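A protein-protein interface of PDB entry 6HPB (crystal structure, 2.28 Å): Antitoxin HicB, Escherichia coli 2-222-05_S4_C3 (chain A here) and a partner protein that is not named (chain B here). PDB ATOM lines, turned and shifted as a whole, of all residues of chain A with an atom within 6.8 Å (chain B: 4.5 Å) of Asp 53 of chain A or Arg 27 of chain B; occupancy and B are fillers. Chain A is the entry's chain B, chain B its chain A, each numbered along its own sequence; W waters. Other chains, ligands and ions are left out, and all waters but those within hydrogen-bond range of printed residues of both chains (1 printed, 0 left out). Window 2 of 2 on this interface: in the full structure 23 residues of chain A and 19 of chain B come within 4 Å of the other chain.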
ATOM      1  N   ASP A  48     -23.516  -4.278  21.655  1.00  0.00           N
ATOM      2  CA  ASP A  48     -24.233  -5.150  20.722  1.00  0.00           C
ATOM      3  C   ASP A  48     -24.306  -6.580  21.240  1.00  0.00           C
ATOM      4  O   ASP A  48     -25.333  -7.252  21.068  1.00  0.00           O
ATOM      5  CB  ASP A  48     -23.598  -5.164  19.333  1.00  0.00           C
ATOM      6  CG  ASP A  48     -23.742  -3.858  18.610  1.00  0.00           C
ATOM      7  OD1 ASP A  48     -24.385  -2.957  19.176  1.00  0.00           O
ATOM      8  OD2 ASP A  48     -23.209  -3.727  17.483  1.00  0.00           O
ATOM      9  N   PHE A  49     -23.228  -7.064  21.876  1.00  0.00           N
ATOM     10  CA  PHE A  49     -23.224  -8.438  22.364  1.00  0.00           C
ATOM     11  C   PHE A  49     -24.418  -8.684  23.271  1.00  0.00           C
ATOM     12  O   PHE A  49     -25.026  -9.755  23.244  1.00  0.00           O
ATOM     13  CB  PHE A  49     -21.958  -8.742  23.152  1.00  0.00           C
ATOM     14  CG  PHE A  49     -20.690  -8.866  22.325  1.00  0.00           C
ATOM     15  CD1 PHE A  49     -20.556  -9.824  21.339  1.00  0.00           C
ATOM     16  CD2 PHE A  49     -19.609  -8.051  22.605  1.00  0.00           C
ATOM     17  CE1 PHE A  49     -19.374  -9.938  20.602  1.00  0.00           C
ATOM     18  CE2 PHE A  49     -18.409  -8.170  21.886  1.00  0.00           C
ATOM     19  CZ  PHE A  49     -18.294  -9.119  20.891  1.00  0.00           C
ATOM     20  N   TYR A  50     -24.690  -7.735  24.153  1.00  0.00           N
ATOM     21  CA  TYR A  50     -25.710  -7.914  25.166  1.00  0.00           C
ATOM     22  C   TYR A  50     -27.105  -7.885  24.550  1.00  0.00           C
ATOM     23  O   TYR A  50     -27.973  -8.683  24.917  1.00  0.00           O
ATOM     24  CB  TYR A  50     -25.539  -6.832  26.241  1.00  0.00           C
ATOM     25  CG  TYR A  50     -24.253  -6.983  27.060  1.00  0.00           C
ATOM     26  CD1 TYR A  50     -23.031  -6.530  26.579  1.00  0.00           C
ATOM     27  CD2 TYR A  50     -24.276  -7.616  28.304  1.00  0.00           C
ATOM     28  CE1 TYR A  50     -21.864  -6.690  27.331  1.00  0.00           C
ATOM     29  CE2 TYR A  50     -23.128  -7.789  29.055  1.00  0.00           C
ATOM     30  CZ  TYR A  50     -21.923  -7.307  28.566  1.00  0.00           C
ATOM     31  OH  TYR A  50     -20.789  -7.493  29.306  1.00  0.00           O
ATOM     32  N   PHE A  51     -27.343  -6.961  23.626  1.00  0.00           N
ATOM     33  CA  PHE A  51     -28.607  -6.985  22.907  1.00  0.00           C
ATOM     34  C   PHE A  51     -28.770  -8.297  22.162  1.00  0.00           C
ATOM     35  O   PHE A  51     -29.843  -8.909  22.206  1.00  0.00           O
ATOM     36  CB  PHE A  51     -28.691  -5.807  21.941  1.00  0.00           C
ATOM     37  CG  PHE A  51     -28.932  -4.488  22.607  1.00  0.00           C
ATOM     38  CD1 PHE A  51     -30.223  -4.057  22.860  1.00  0.00           C
ATOM     39  CD2 PHE A  51     -27.873  -3.672  22.981  1.00  0.00           C
ATOM     40  CE1 PHE A  51     -30.460  -2.840  23.464  1.00  0.00           C
ATOM     41  CE2 PHE A  51     -28.117  -2.430  23.582  1.00  0.00           C
ATOM     42  CZ  PHE A  51     -29.397  -2.033  23.837  1.00  0.00           C
ATOM     43  N   GLU A  52     -27.687  -8.798  21.548  1.00  0.00           N
ATOM     44  CA  GLU A  52     -27.817 -10.026  20.770  1.00  0.00           C
ATOM     45  C   GLU A  52     -28.072 -11.208  21.683  1.00  0.00           C
ATOM     46  O   GLU A  52     -28.892 -12.077  21.372  1.00  0.00           O
ATOM     47  CB  GLU A  52     -26.578 -10.292  19.908  1.00  0.00           C
ATOM     48  CG  GLU A  52     -26.273  -9.246  18.852  1.00  0.00           C
ATOM     49  CD  GLU A  52     -24.885  -9.412  18.205  1.00  0.00           C
ATOM     50  OE1 GLU A  52     -24.307 -10.532  18.246  1.00  0.00           O
ATOM     51  OE2 GLU A  52     -24.375  -8.404  17.660  1.00  0.00           O
ATOM     52  N   ASP A  53     -27.360 -11.287  22.808  1.00  0.00           N
ATOM     53  CA  ASP A  53     -27.485 -12.459  23.666  1.00  0.00           C
ATOM     54  C   ASP A  53     -28.568 -12.300  24.711  1.00  0.00           C
ATOM     55  O   ASP A  53     -28.724 -13.183  25.557  1.00  0.00           O
ATOM     56  CB  ASP A  53     -26.160 -12.765  24.344  1.00  0.00           C
ATOM     57  CG  ASP A  53     -25.074 -13.083  23.352  1.00  0.00           C
ATOM     58  OD1 ASP A  53     -25.390 -13.287  22.172  1.00  0.00           O
ATOM     59  OD2 ASP A  53     -23.899 -13.112  23.760  1.00  0.00           O
ATOM     60  N   ASN A  54     -29.319 -11.206  24.667  1.00  0.00           N
ATOM     61  CA  ASN A  54     -30.383 -10.986  25.626  1.00  0.00           C
ATOM     62  C   ASN A  54     -29.853 -11.110  27.040  1.00  0.00           C
ATOM     63  O   ASN A  54     -30.391 -11.861  27.841  1.00  0.00           O
ATOM     64  CB  ASN A  54     -31.536 -11.969  25.398  1.00  0.00           C
ATOM     65  CG  ASN A  54     -32.210 -11.760  24.057  1.00  0.00           C
ATOM     66  OD1 ASN A  54     -32.199 -12.645  23.199  1.00  0.00           O
ATOM     67  ND2 ASN A  54     -32.763 -10.577  23.857  1.00  0.00           N
ATOM     68  N   GLU A  55     -28.782 -10.367  27.355  1.00  0.00           N
ATOM     69  CA  GLU A  55     -28.229 -10.368  28.701  1.00  0.00           C
ATOM     70  C   GLU A  55     -28.265  -8.946  29.248  1.00  0.00           C
ATOM     71  O   GLU A  55     -28.160  -7.987  28.488  1.00  0.00           O
ATOM     72  CB  GLU A  55     -26.772 -10.950  28.670  1.00  0.00           C
ATOM     73  CG  GLU A  55     -25.797 -10.493  29.735  1.00  0.00           C
ATOM     74  CD  GLU A  55     -24.447 -11.293  29.696  1.00  0.00           C
ATOM     75  OE1 GLU A  55     -24.200 -11.976  28.679  1.00  0.00           O
ATOM     76  OE2 GLU A  55     -23.629 -11.208  30.652  1.00  0.00           O
ATOM     77  N   LEU A  56     -28.475  -8.804  30.554  1.00  0.00           N
ATOM     78  CA  LEU A  56     -28.459  -7.480  31.177  1.00  0.00           C
ATOM     79  C   LEU A  56     -27.138  -6.759  30.922  1.00  0.00           C
ATOM     80  O   LEU A  56     -26.056  -7.349  31.008  1.00  0.00           O
ATOM     81  CB  LEU A  56     -28.714  -7.596  32.686  1.00  0.00           C
ATOM     82  CG  LEU A  56     -30.089  -8.204  33.045  1.00  0.00           C
ATOM     83  CD1 LEU A  56     -30.050  -8.791  34.449  1.00  0.00           C
ATOM     84  CD2 LEU A  56     -31.240  -7.193  32.883  1.00  0.00           C
ATOM     85  N   LEU A  87     -35.645  -7.351  29.631  1.00  0.00           N
ATOM     86  CA  LEU A  87     -35.178  -8.673  30.030  1.00  0.00           C
ATOM     87  C   LEU A  87     -35.720  -9.032  31.403  1.00  0.00           C
ATOM     88  O   LEU A  87     -36.083 -10.185  31.653  1.00  0.00           O
ATOM     89  CB  LEU A  87     -33.648  -8.747  30.005  1.00  0.00           C
ATOM     90  CG  LEU A  87     -33.059  -8.532  28.611  1.00  0.00           C
ATOM     91  CD1 LEU A  87     -31.533  -8.375  28.672  1.00  0.00           C
ATOM     92  CD2 LEU A  87     -33.451  -9.681  27.724  1.00  0.00           C
ATOM     93  N   VAL B  15     -11.988 -18.644  16.574  1.00  0.00           N
ATOM     94  CA  VAL B  15     -12.678 -17.465  16.990  1.00  0.00           C
ATOM     95  C   VAL B  15     -13.404 -16.928  15.798  1.00  0.00           C
ATOM     96  O   VAL B  15     -12.891 -16.988  14.741  1.00  0.00           O
ATOM     97  CB  VAL B  15     -11.672 -16.418  17.480  1.00  0.00           C
ATOM     98  CG1 VAL B  15     -12.347 -15.140  17.873  1.00  0.00           C
ATOM     99  CG2 VAL B  15     -10.910 -16.924  18.661  1.00  0.00           C
ATOM    100  N   ASP B  16     -14.624 -16.452  15.977  1.00  0.00           N
ATOM    101  CA  ASP B  16     -15.424 -15.863  14.911  1.00  0.00           C
ATOM    102  C   ASP B  16     -15.400 -14.352  14.959  1.00  0.00           C
ATOM    103  O   ASP B  16     -15.586 -13.761  15.966  1.00  0.00           O
ATOM    104  CB  ASP B  16     -16.852 -16.403  14.956  1.00  0.00           C
ATOM    105  CG  ASP B  16     -17.852 -15.521  14.258  1.00  0.00           C
ATOM    106  OD1 ASP B  16     -18.378 -14.617  14.865  1.00  0.00           O
ATOM    107  OD2 ASP B  16     -18.161 -15.731  13.104  1.00  0.00           O
ATOM    108  N   LYS B  25     -16.019  -7.579  16.492  1.00  0.00           N
ATOM    109  CA  LYS B  25     -16.725  -8.352  17.512  1.00  0.00           C
ATOM    110  C   LYS B  25     -16.257  -9.810  17.458  1.00  0.00           C
ATOM    111  O   LYS B  25     -16.412 -10.476  16.429  1.00  0.00           O
ATOM    112  CB  LYS B  25     -18.229  -8.231  17.324  1.00  0.00           C
ATOM    113  CG  LYS B  25     -18.821  -6.987  17.948  1.00  0.00           C
ATOM    114  CD  LYS B  25     -19.724  -6.215  16.967  1.00  0.00           C
ATOM    115  CE  LYS B  25     -21.058  -6.882  16.772  1.00  0.00           C
ATOM    116  NZ  LYS B  25     -22.123  -5.956  16.248  1.00  0.00           N
ATOM    117  N   LEU B  26     -15.611 -10.273  18.528  1.00  0.00           N
ATOM    118  CA  LEU B  26     -15.021 -11.610  18.599  1.00  0.00           C
ATOM    119  C   LEU B  26     -15.837 -12.516  19.516  1.00  0.00           C
ATOM    120  O   LEU B  26     -16.233 -12.105  20.612  1.00  0.00           O
ATOM    121  CB  LEU B  26     -13.576 -11.538  19.101  1.00  0.00           C
ATOM    122  CG  LEU B  26     -12.716 -10.507  18.358  1.00  0.00           C
ATOM    123  CD1 LEU B  26     -11.451 -10.205  19.130  1.00  0.00           C
ATOM    124  CD2 LEU B  26     -12.382 -10.955  16.937  1.00  0.00           C
ATOM    125  N   ARG B  27     -16.147 -13.712  19.040  1.00  0.00           N
ATOM    126  CA  ARG B  27     -16.876 -14.691  19.834  1.00  0.00           C
ATOM    127  C   ARG B  27     -16.125 -16.013  19.841  1.00  0.00           C
ATOM    128  O   ARG B  27     -15.584 -16.428  18.814  1.00  0.00           O
ATOM    129  CB  ARG B  27     -18.291 -14.877  19.314  1.00  0.00           C
ATOM    130  CG  ARG B  27     -19.281 -13.802  19.788  1.00  0.00           C
ATOM    131  CD  ARG B  27     -20.633 -14.005  19.075  1.00  0.00           C
ATOM    132  NE  ARG B  27     -21.654 -13.017  19.425  1.00  0.00           N
ATOM    133  CZ  ARG B  27     -22.376 -13.044  20.544  1.00  0.00           C
ATOM    134  NH1 ARG B  27     -22.170 -14.006  21.447  1.00  0.00           N
ATOM    135  NH2 ARG B  27     -23.303 -12.110  20.764  1.00  0.00           N
ATOM    136  N   PHE B  28     -16.035 -16.639  21.016  1.00  0.00           N
ATOM    137  CA  PHE B  28     -15.285 -17.889  21.166  1.00  0.00           C
ATOM    138  C   PHE B  28     -15.856 -18.716  22.309  1.00  0.00           C
ATOM    139  O   PHE B  28     -15.640 -18.363  23.476  1.00  0.00           O
ATOM    140  CB  PHE B  28     -13.800 -17.635  21.391  1.00  0.00           C
ATOM    141  CG  PHE B  28     -12.970 -18.882  21.259  1.00  0.00           C
ATOM    142  CD1 PHE B  28     -13.045 -19.647  20.110  1.00  0.00           C
ATOM    143  CD2 PHE B  28     -12.164 -19.313  22.295  1.00  0.00           C
ATOM    144  CE1 PHE B  28     -12.304 -20.796  19.975  1.00  0.00           C
ATOM    145  CE2 PHE B  28     -11.426 -20.473  22.174  1.00  0.00           C
ATOM    146  CZ  PHE B  28     -11.493 -21.211  21.009  1.00  0.00           C
ATOM    147  N   HIS B  29     -16.571 -19.798  21.987  1.00  0.00           N
ATOM    148  CA  HIS B  29     -17.085 -20.732  23.001  1.00  0.00           C
ATOM    149  C   HIS B  29     -17.839 -19.995  24.101  1.00  0.00           C
ATOM    150  O   HIS B  29     -17.560 -20.157  25.288  1.00  0.00           O
ATOM    151  CB  HIS B  29     -15.953 -21.541  23.639  1.00  0.00           C
ATOM    152  CG  HIS B  29     -15.292 -22.526  22.727  1.00  0.00           C
ATOM    153  ND1 HIS B  29     -14.579 -22.153  21.609  1.00  0.00           N
ATOM    154  CD2 HIS B  29     -15.206 -23.875  22.793  1.00  0.00           C
ATOM    155  CE1 HIS B  29     -14.102 -23.231  21.013  1.00  0.00           C
ATOM    156  NE2 HIS B  29     -14.462 -24.287  21.715  1.00  0.00           N
ATOM    157  N   ARG B  31     -17.649 -16.928  24.872  1.00  0.00           N
ATOM    158  CA  ARG B  31     -16.981 -15.720  25.320  1.00  0.00           C
ATOM    159  C   ARG B  31     -16.919 -14.713  24.184  1.00  0.00           C
ATOM    160  O   ARG B  31     -17.006 -15.052  23.005  1.00  0.00           O
ATOM    161  CB  ARG B  31     -15.593 -16.037  25.875  1.00  0.00           C
ATOM    162  CG  ARG B  31     -15.719 -16.782  27.214  1.00  0.00           C
ATOM    163  CD  ARG B  31     -14.397 -17.087  27.868  1.00  0.00           C
ATOM    164  NE  ARG B  31     -14.147 -16.260  29.050  1.00  0.00           N
ATOM    165  CZ  ARG B  31     -13.981 -16.743  30.280  1.00  0.00           C
ATOM    166  NH1 ARG B  31     -14.053 -18.051  30.502  1.00  0.00           N
ATOM    167  NH2 ARG B  31     -13.746 -15.917  31.291  1.00  0.00           N
ATOM    168  N   ARG B  32     -16.891 -13.461  24.570  1.00  0.00           N
ATOM    169  CA  ARG B  32     -17.048 -12.343  23.666  1.00  0.00           C
ATOM    170  C   ARG B  32     -15.996 -11.309  24.005  1.00  0.00           C
ATOM    171  O   ARG B  32     -15.645 -11.140  25.174  1.00  0.00           O
ATOM    172  CB  ARG B  32     -18.457 -11.742  23.797  1.00  0.00           C
ATOM    173  CG  ARG B  32     -19.549 -12.777  23.576  1.00  0.00           C
ATOM    174  CD  ARG B  32     -20.908 -12.353  24.101  1.00  0.00           C
ATOM    175  NE  ARG B  32     -20.849 -11.608  25.356  1.00  0.00           N
ATOM    176  CZ  ARG B  32     -21.892 -11.431  26.165  1.00  0.00           C
ATOM    177  NH1 ARG B  32     -23.078 -11.944  25.846  1.00  0.00           N
ATOM    178  NH2 ARG B  32     -21.748 -10.756  27.299  1.00  0.00           N
HETATM  179  O   HOH W   1     -20.975 -11.060  17.502  1.00  0.00           O
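The side-chain amino group (NZ) of Lys 25 of chain B is in salt-bridge range of the side-chain carboxylate (OD2) of Asp 48 of chain A, at 2.8 Å. The guanidinium group of Arg 32 of chain B is in salt-bridge range of the side-chain carboxylate of Glu 55 of chain A (3.0 Å). The side-chain carboxylate of Asp 53 of chain A is in salt-bridge range of the guanidinium group of Arg 27 of chain B (2.8 Å). NZ of Lys 25 of chain B is in salt-bridge range of OE2 of Glu 52 of chain A. The guanidinium group (NH2) of Arg 27 of chain B lies within salt-bridge range of the side-chain carboxylate (OE1) of Glu 52 of chain A, at 3.1 Å. OD2 of Asp 53 of chain A is in salt-bridge range of NH1 of Arg 32 of chain B (2.5 Å).
The backbone NH of Asp 16 of chain B sits at hydrogen-bond distance from the backbone carbonyl oxygen of Arg 27 of chain B, 3.0 Å away. The backbone NH (N) of Glu 55 of chain A lies within hydrogen-bond range of the backbone carbonyl oxygen (O) of Tyr 50 of chain A.
Phe 49 of chain A touches Lys 25 of chain B. CZ of Phe 49 of chain A touches O of Leu 26 of chain B (3.6 Å). Phe 49 of chain A touches Arg 27 of chain B. Phe 49 of chain A touches Arg 32 of chain B. Arg 32 of chain B touches Tyr 50 of chain A (NH2 to CZ, 3.7 Å).
Arg 27 of chain B touches just these residues of chain A: Phe 49 (3.6 Å), Glu 52 (3.1 Å) and Asp 53 (2.8 Å). Printed residues of chain B within 4 Å of Phe 49 of chain A: Lys 25 (3.7 Å), Leu 26 (3.6 Å), Arg 27 (3.6 Å) and Arg 32 (3.8 Å). Of the printed residues of chain A, Arg 32 of chain B touches Phe 49 (3.8 Å), Tyr 50 (3.7 Å), Asp 53 (2.5 Å) and Glu 55 (3.0 Å). Asp 16 of chain B touches none of the printed residues of chain A. Arg 31 of chain B touches none of the printed residues of chain A. The nearest printed residue of chain A that does not touch Lys 25 of chain B is Tyr 50 of chain A (8.3 Å).
Of the 10 printed residues of chain A, 6 touch a printed residue of chain B. Hydrophobic or aromatic side chains of chain A within 4 Å of the printed part of chain B: Phe 49 and Tyr 50.
Water W1 lies within hydrogen-bond range of the guanidinium group (NE) of Arg 27 of chain B (2.8 Å) and the side-chain carboxylate (OE1) of Glu 52 of chain A (3.5 Å).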
